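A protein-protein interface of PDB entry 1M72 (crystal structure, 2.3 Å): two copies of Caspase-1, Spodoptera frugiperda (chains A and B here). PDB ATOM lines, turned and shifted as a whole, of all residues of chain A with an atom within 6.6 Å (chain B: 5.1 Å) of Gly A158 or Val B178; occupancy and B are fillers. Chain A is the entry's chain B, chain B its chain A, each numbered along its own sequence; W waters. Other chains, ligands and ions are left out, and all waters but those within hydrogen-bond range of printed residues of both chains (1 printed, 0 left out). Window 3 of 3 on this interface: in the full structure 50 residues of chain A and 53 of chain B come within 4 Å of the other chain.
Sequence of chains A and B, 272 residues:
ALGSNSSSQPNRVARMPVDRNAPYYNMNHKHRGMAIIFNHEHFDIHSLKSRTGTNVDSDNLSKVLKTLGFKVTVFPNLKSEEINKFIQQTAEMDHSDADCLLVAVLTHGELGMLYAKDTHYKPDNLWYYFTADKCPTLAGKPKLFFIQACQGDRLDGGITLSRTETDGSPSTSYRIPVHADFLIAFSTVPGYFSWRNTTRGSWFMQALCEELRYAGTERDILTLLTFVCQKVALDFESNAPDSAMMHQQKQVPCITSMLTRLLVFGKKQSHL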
ATOM      1  N   LEU A 155      34.365  20.030   1.310  1.00  0.00           N
ATOM      2  CA  LEU A 155      33.302  21.038   1.294  1.00  0.00           C
ATOM      3  C   LEU A 155      32.548  20.985   2.584  1.00  0.00           C
ATOM      4  O   LEU A 155      32.455  19.933   3.177  1.00  0.00           O
ATOM      5  CB  LEU A 155      32.310  20.796   0.149  1.00  0.00           C
ATOM      6  CG  LEU A 155      32.871  20.937  -1.258  1.00  0.00           C
ATOM      7  CD1 LEU A 155      31.999  20.182  -2.211  1.00  0.00           C
ATOM      8  CD2 LEU A 155      32.974  22.403  -1.623  1.00  0.00           C
ATOM      9  N   ASP A 156      32.025  22.132   3.013  1.00  0.00           N
ATOM     10  CA  ASP A 156      31.263  22.240   4.263  1.00  0.00           C
ATOM     11  C   ASP A 156      29.822  22.608   3.851  1.00  0.00           C
ATOM     12  O   ASP A 156      29.528  23.765   3.494  1.00  0.00           O
ATOM     13  CB  ASP A 156      31.884  23.331   5.161  1.00  0.00           C
ATOM     14  CG  ASP A 156      31.240  23.401   6.563  1.00  0.00           C
ATOM     15  OD1 ASP A 156      29.987  23.268   6.669  1.00  0.00           O
ATOM     16  OD2 ASP A 156      31.987  23.591   7.565  1.00  0.00           O
ATOM     17  N   GLY A 157      28.939  21.612   3.892  1.00  0.00           N
ATOM     18  CA  GLY A 157      27.564  21.834   3.484  1.00  0.00           C
ATOM     19  C   GLY A 157      26.751  22.689   4.448  1.00  0.00           C
ATOM     20  O   GLY A 157      25.597  23.027   4.170  1.00  0.00           O
ATOM     21  N   GLY A 158      27.359  23.036   5.581  1.00  0.00           N
ATOM     22  CA  GLY A 158      26.672  23.838   6.580  1.00  0.00           C
ATOM     23  C   GLY A 158      25.450  23.154   7.178  1.00  0.00           C
ATOM     24  O   GLY A 158      25.080  22.055   6.788  1.00  0.00           O
ATOM     25  N   ILE A 159      24.818  23.803   8.146  1.00  0.00           N
ATOM     26  CA  ILE A 159      23.610  23.258   8.751  1.00  0.00           C
ATOM     27  C   ILE A 159      22.726  24.451   9.082  1.00  0.00           C
ATOM     28  O   ILE A 159      23.239  25.522   9.420  1.00  0.00           O
ATOM     29  CB  ILE A 159      23.895  22.495  10.063  1.00  0.00           C
ATOM     30  CG1 ILE A 159      22.568  21.966  10.648  1.00  0.00           C
ATOM     31  CG2 ILE A 159      24.569  23.434  11.069  1.00  0.00           C
ATOM     32  CD1 ILE A 159      22.703  21.036  11.881  1.00  0.00           C
ATOM     33  N   THR A 160      21.410  24.269   8.995  1.00  0.00           N
ATOM     34  CA  THR A 160      20.463  25.333   9.297  1.00  0.00           C
ATOM     35  C   THR A 160      20.081  25.269  10.772  1.00  0.00           C
ATOM     36  O   THR A 160      19.840  24.187  11.301  1.00  0.00           O
ATOM     37  CB  THR A 160      19.197  25.201   8.410  1.00  0.00           C
ATOM     38  OG1 THR A 160      19.584  25.272   7.034  1.00  0.00           O
ATOM     39  CG2 THR A 160      18.200  26.335   8.673  1.00  0.00           C
ATOM     40  N   TYR A 192      39.982  21.985   3.700  1.00  0.00           N
ATOM     41  CA  TYR A 192      38.850  22.579   2.981  1.00  0.00           C
ATOM     42  C   TYR A 192      39.102  23.594   1.909  1.00  0.00           C
ATOM     43  O   TYR A 192      40.149  24.239   1.868  1.00  0.00           O
ATOM     44  CB  TYR A 192      37.866  23.210   3.978  1.00  0.00           C
ATOM     45  CG  TYR A 192      37.169  22.159   4.753  1.00  0.00           C
ATOM     46  CD1 TYR A 192      37.882  21.391   5.685  1.00  0.00           C
ATOM     47  CD2 TYR A 192      35.867  21.751   4.399  1.00  0.00           C
ATOM     48  CE1 TYR A 192      37.338  20.225   6.225  1.00  0.00           C
ATOM     49  CE2 TYR A 192      35.309  20.602   4.923  1.00  0.00           C
ATOM     50  CZ  TYR A 192      36.054  19.820   5.833  1.00  0.00           C
ATOM     51  OH  TYR A 192      35.579  18.590   6.267  1.00  0.00           O
ATOM     52  N   GLN A 248      25.740  26.223  -2.426  1.00  0.00           N
ATOM     53  CA  GLN A 248      25.273  26.503  -1.069  1.00  0.00           C
ATOM     54  C   GLN A 248      26.229  25.995  -0.024  1.00  0.00           C
ATOM     55  O   GLN A 248      25.806  25.477   0.999  1.00  0.00           O
ATOM     56  CB  GLN A 248      23.896  25.870  -0.830  1.00  0.00           C
ATOM     57  CG  GLN A 248      22.837  26.314  -1.854  1.00  0.00           C
ATOM     58  CD  GLN A 248      21.469  25.747  -1.540  1.00  0.00           C
ATOM     59  OE1 GLN A 248      20.673  25.524  -2.438  1.00  0.00           O
ATOM     60  NE2 GLN A 248      21.192  25.510  -0.253  1.00  0.00           N
ATOM     61  N   GLN A 249      27.521  26.133  -0.283  1.00  0.00           N
ATOM     62  CA  GLN A 249      28.503  25.663   0.680  1.00  0.00           C
ATOM     63  C   GLN A 249      28.888  26.806   1.626  1.00  0.00           C
ATOM     64  O   GLN A 249      28.688  27.990   1.312  1.00  0.00           O
ATOM     65  CB  GLN A 249      29.711  25.074  -0.054  1.00  0.00           C
ATOM     66  CG  GLN A 249      29.301  23.971  -1.048  1.00  0.00           C
ATOM     67  CD  GLN A 249      28.756  22.750  -0.337  1.00  0.00           C
ATOM     68  OE1 GLN A 249      29.477  22.112   0.414  1.00  0.00           O
ATOM     69  NE2 GLN A 249      27.471  22.435  -0.552  1.00  0.00           N
ATOM     70  N   LYS A 250      29.405  26.423   2.787  1.00  0.00           N
ATOM     71  CA  LYS A 250      29.791  27.328   3.872  1.00  0.00           C
ATOM     72  C   LYS A 250      31.283  27.263   4.134  1.00  0.00           C
ATOM     73  O   LYS A 250      31.999  26.386   3.602  1.00  0.00           O
ATOM     74  CB  LYS A 250      29.062  26.920   5.137  1.00  0.00           C
ATOM     75  CG  LYS A 250      27.559  26.893   4.958  1.00  0.00           C
ATOM     76  CD  LYS A 250      27.018  28.301   4.782  1.00  0.00           C
ATOM     77  CE  LYS A 250      26.875  28.990   6.159  1.00  0.00           C
ATOM     78  NZ  LYS A 250      26.678  30.439   5.969  1.00  0.00           N
ATOM     79  N   VAL A 252      34.393  28.547   7.330  1.00  0.00           N
ATOM     80  CA  VAL A 252      34.818  29.225   8.545  1.00  0.00           C
ATOM     81  C   VAL A 252      36.359  29.309   8.543  1.00  0.00           C
ATOM     82  O   VAL A 252      37.040  28.369   8.153  1.00  0.00           O
ATOM     83  CB  VAL A 252      34.298  28.553   9.861  1.00  0.00           C
ATOM     84  CG1 VAL A 252      34.964  27.148  10.111  1.00  0.00           C
ATOM     85  CG2 VAL A 252      34.586  29.488  11.042  1.00  0.00           C
ATOM     86  N   ARG B  12      20.676  20.825   6.744  1.00  0.00           N
ATOM     87  CA  ARG B  12      20.116  19.949   7.843  1.00  0.00           C
ATOM     88  C   ARG B  12      19.553  20.901   8.900  1.00  0.00           C
ATOM     89  O   ARG B  12      19.717  22.110   8.753  1.00  0.00           O
ATOM     90  CB  ARG B  12      21.229  19.035   8.457  1.00  0.00           C
ATOM     91  N   THR B 131      31.267  17.592  14.569  1.00  0.00           N
ATOM     92  CA  THR B 131      30.877  18.648  13.626  1.00  0.00           C
ATOM     93  C   THR B 131      29.334  18.720  13.692  1.00  0.00           C
ATOM     94  O   THR B 131      28.652  17.697  13.898  1.00  0.00           O
ATOM     95  CB  THR B 131      31.369  18.336  12.201  1.00  0.00           C
ATOM     96  OG1 THR B 131      31.098  16.968  11.909  1.00  0.00           O
ATOM     97  CG2 THR B 131      32.886  18.583  12.069  1.00  0.00           C
ATOM     98  N   ALA B 132      28.807  19.935  13.567  1.00  0.00           N
ATOM     99  CA  ALA B 132      27.368  20.219  13.660  1.00  0.00           C
ATOM    100  C   ALA B 132      26.481  19.157  12.983  1.00  0.00           C
ATOM    101  O   ALA B 132      25.428  18.783  13.524  1.00  0.00           O
ATOM    102  CB  ALA B 132      27.065  21.635  13.079  1.00  0.00           C
ATOM    103  N   ASP B 133      26.893  18.685  11.812  1.00  0.00           N
ATOM    104  CA  ASP B 133      26.130  17.661  11.110  1.00  0.00           C
ATOM    105  C   ASP B 133      26.139  16.348  11.876  1.00  0.00           C
ATOM    106  O   ASP B 133      25.178  15.600  11.811  1.00  0.00           O
ATOM    107  CB  ASP B 133      26.671  17.425   9.688  1.00  0.00           C
ATOM    108  CG  ASP B 133      28.149  17.056   9.665  1.00  0.00           C
ATOM    109  OD1 ASP B 133      28.869  17.385  10.611  1.00  0.00           O
ATOM    110  OD2 ASP B 133      28.608  16.451   8.684  1.00  0.00           O
ATOM    111  N   ARG B 175      21.941  29.698   8.696  1.00  0.00           N
ATOM    112  CA  ARG B 175      22.907  28.634   8.425  1.00  0.00           C
ATOM    113  C   ARG B 175      24.352  28.909   8.821  1.00  0.00           C
ATOM    114  O   ARG B 175      24.871  29.997   8.573  1.00  0.00           O
ATOM    115  CB  ARG B 175      22.858  28.244   6.947  1.00  0.00           C
ATOM    116  CG  ARG B 175      21.616  27.436   6.636  1.00  0.00           C
ATOM    117  CD  ARG B 175      21.366  27.278   5.175  1.00  0.00           C
ATOM    118  NE  ARG B 175      22.524  26.761   4.467  1.00  0.00           N
ATOM    119  CZ  ARG B 175      23.047  25.542   4.595  1.00  0.00           C
ATOM    120  NH1 ARG B 175      22.525  24.627   5.428  1.00  0.00           N
ATOM    121  NH2 ARG B 175      24.113  25.256   3.862  1.00  0.00           N
ATOM    122  N   ILE B 176      24.980  27.895   9.426  1.00  0.00           N
ATOM    123  CA  ILE B 176      26.384  27.945   9.856  1.00  0.00           C
ATOM    124  C   ILE B 176      27.244  26.814   9.291  1.00  0.00           C
ATOM    125  O   ILE B 176      26.729  25.750   8.940  1.00  0.00           O
ATOM    126  CB  ILE B 176      26.520  27.887  11.388  1.00  0.00           C
ATOM    127  CG1 ILE B 176      26.203  26.477  11.902  1.00  0.00           C
ATOM    128  CG2 ILE B 176      25.598  28.909  12.009  1.00  0.00           C
ATOM    129  CD1 ILE B 176      26.499  26.313  13.411  1.00  0.00           C
ATOM    130  N   PRO B 177      28.569  27.030   9.203  1.00  0.00           N
ATOM    131  CA  PRO B 177      29.448  25.970   8.673  1.00  0.00           C
ATOM    132  C   PRO B 177      29.475  24.856   9.750  1.00  0.00           C
ATOM    133  O   PRO B 177      29.454  25.159  10.951  1.00  0.00           O
ATOM    134  CB  PRO B 177      30.825  26.672   8.509  1.00  0.00           C
ATOM    135  CG  PRO B 177      30.494  28.161   8.579  1.00  0.00           C
ATOM    136  CD  PRO B 177      29.325  28.252   9.522  1.00  0.00           C
ATOM    137  N   VAL B 178      29.490  23.586   9.344  1.00  0.00           N
ATOM    138  CA  VAL B 178      29.493  22.523  10.350  1.00  0.00           C
ATOM    139  C   VAL B 178      30.834  22.405  11.073  1.00  0.00           C
ATOM    140  O   VAL B 178      30.914  21.759  12.093  1.00  0.00           O
ATOM    141  CB  VAL B 178      29.062  21.153   9.744  1.00  0.00           C
ATOM    142  CG1 VAL B 178      27.757  21.366   8.898  1.00  0.00           C
ATOM    143  CG2 VAL B 178      30.233  20.489   8.930  1.00  0.00           C
ATOM    144  N   HIS B 179      31.889  23.045  10.559  1.00  0.00           N
ATOM    145  CA  HIS B 179      33.203  23.003  11.232  1.00  0.00           C
ATOM    146  C   HIS B 179      33.422  24.228  12.109  1.00  0.00           C
ATOM    147  O   HIS B 179      34.514  24.403  12.646  1.00  0.00           O
ATOM    148  CB  HIS B 179      34.348  22.929  10.217  1.00  0.00           C
ATOM    149  CG  HIS B 179      34.447  21.606   9.538  1.00  0.00           C
ATOM    150  ND1 HIS B 179      35.017  20.505  10.144  1.00  0.00           N
ATOM    151  CD2 HIS B 179      34.005  21.188   8.326  1.00  0.00           C
ATOM    152  CE1 HIS B 179      34.921  19.466   9.330  1.00  0.00           C
ATOM    153  NE2 HIS B 179      34.313  19.852   8.221  1.00  0.00           N
ATOM    154  N   ALA B 180      32.404  25.076  12.260  1.00  0.00           N
ATOM    155  CA  ALA B 180      32.584  26.258  13.093  1.00  0.00           C
ATOM    156  C   ALA B 180      32.411  25.954  14.558  1.00  0.00           C
ATOM    157  O   ALA B 180      31.829  24.945  14.921  1.00  0.00           O
ATOM    158  CB  ALA B 180      31.602  27.361  12.693  1.00  0.00           C
ATOM    159  N   PHE B 182      34.803  25.463  17.062  1.00  0.00           N
ATOM    160  CA  PHE B 182      35.741  24.586  17.704  1.00  0.00           C
ATOM    161  C   PHE B 182      36.914  25.425  18.188  1.00  0.00           C
ATOM    162  O   PHE B 182      37.366  26.373  17.504  1.00  0.00           O
ATOM    163  CB  PHE B 182      36.294  23.532  16.727  1.00  0.00           C
ATOM    164  CG  PHE B 182      35.359  22.397  16.465  1.00  0.00           C
ATOM    165  CD1 PHE B 182      35.536  21.177  17.104  1.00  0.00           C
ATOM    166  CD2 PHE B 182      34.313  22.541  15.543  1.00  0.00           C
ATOM    167  CE1 PHE B 182      34.694  20.097  16.842  1.00  0.00           C
ATOM    168  CE2 PHE B 182      33.463  21.477  15.271  1.00  0.00           C
ATOM    169  CZ  PHE B 182      33.654  20.247  15.923  1.00  0.00           C
HETATM  170  O   HOH W   1      24.249  22.935   1.247  1.00  0.00           O
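No position is printed for both chains.
Gly A158 touches just these residues of chain B: Arg B175 (3.7 Å), Ile B176 (3.0 Å) and Val B178 (3.4 Å).
Of the printed residues of chain B, Gln A248 touches Arg B175 (3.3 Å).
Of the printed residues of chain A, Ile B176 touches Gly A158 (3.0 Å), Ile A159 (2.8 Å) and Lys A250 (3.8 Å).
Printed residues of chain A within 4 Å of Pro B177: Asp A156 and Lys A250.
Printed residues of chain A within 4 Å of His B179: Asp A156, Tyr A192 and Val A252.
The nearest residue of chain A that does not touch Val B178 is Gly A157 (4.8 Å).
The nearest printed residue of chain A that does not touch Ile B176 is Asp A156 (4.7 Å).
NH1 of Arg B175 lies close to OG1 of Thr A160 (3.4 Å).
The side-chain hydroxyl (OH) of Tyr A192 sits at hydrogen-bond distance from a ring nitrogen (NE2) of His B179.
The guanidinium group (NH2) of Arg B175 is in hydrogen-bond range of the backbone carbonyl oxygen (O) of Gly A157 (2.7 Å).
The guanidinium group of Arg B175 lies within hydrogen-bond range of the backbone carbonyl oxygen of Gln A248, at 3.3 Å.
The side-chain carboxylate (OD2) of Asp A156 lies within hydrogen-bond range of the backbone NH (N) of His B179 (3.0 Å).
O of Arg B175 is in hydrogen-bond range of NZ of Lys A250.
O of Ile B176 is in hydrogen-bond range of N of Ile A159, 2.8 Å away.
N of Val B178 sits at hydrogen-bond distance from OD1 of Asp A156 (2.7 Å).
The backbone carbonyl oxygen of Arg B12 sits at hydrogen-bond distance from the backbone NH of Thr A160.
The backbone NH of Lys A250 sits at hydrogen-bond distance from the backbone carbonyl oxygen of Asp A156, 2.8 Å away.
The backbone NH of Ala B132 is in hydrogen-bond range of the backbone carbonyl oxygen of Val B178 (3.2 Å).
OD1 of Asp A156 sits at hydrogen-bond distance from N of Gly A158 (2.9 Å).
The backbone carbonyl oxygen (O) of Asp A156 sits close to the side-chain amide oxygen (OE1) of Gln A249, at 3.5 Å.
Water W1 lies within hydrogen-bond range of O of Gln A248, O of Gly A157 and NH2 of Arg B175.
OD1 of Asp A156 touches CA of Pro B177, at 3.4 Å.
Gly A158 touches Ile B176 (CA to O, 3.0 Å).
CG1 of Val B178 touches C of Gly A158, 3.4 Å away.
Ile A159 touches Arg B12.
CG2 of Ile A159 touches CB of Ala B132 (3.7 Å).
O of Ile A159 touches CA of Arg B175, at 3.3 Å.
Val B178 touches Ile A159.
Ile B176 touches Lys A250 (C to CE, 3.8 Å).
Lys A250 touches Pro B177.
Ala B180 touches Val A252.
Printed residues of chain A that touch a printed residue of chain B: Asp A156, Gly A157, Gly A158, Ile A159, Thr A160, Tyr A192, Gln A248, Lys A250 and Val A252.
Hydrophobic or aromatic side chains of chain A within 4 Å of the printed part of chain B: Ile A159, Tyr A192 and Val A252.
Printed residues of chain B that touch a printed residue of chain A: Arg B12, Ala B132, Arg B175, Ile B176, Pro B177, Val B178, His B179 and Ala B180.
Hydrophobic or aromatic side chains of chain B within 4 Å of the printed part of chain A: Ala B132, Ile B176, Pro B177, Val B178 and His B179.
Among the printed residues, 21 pairs touch across the chains.
Among the printed residues, no Asp or Glu carboxylate lies within 4 Å of a Lys or Arg side-chain nitrogen of the other chain.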
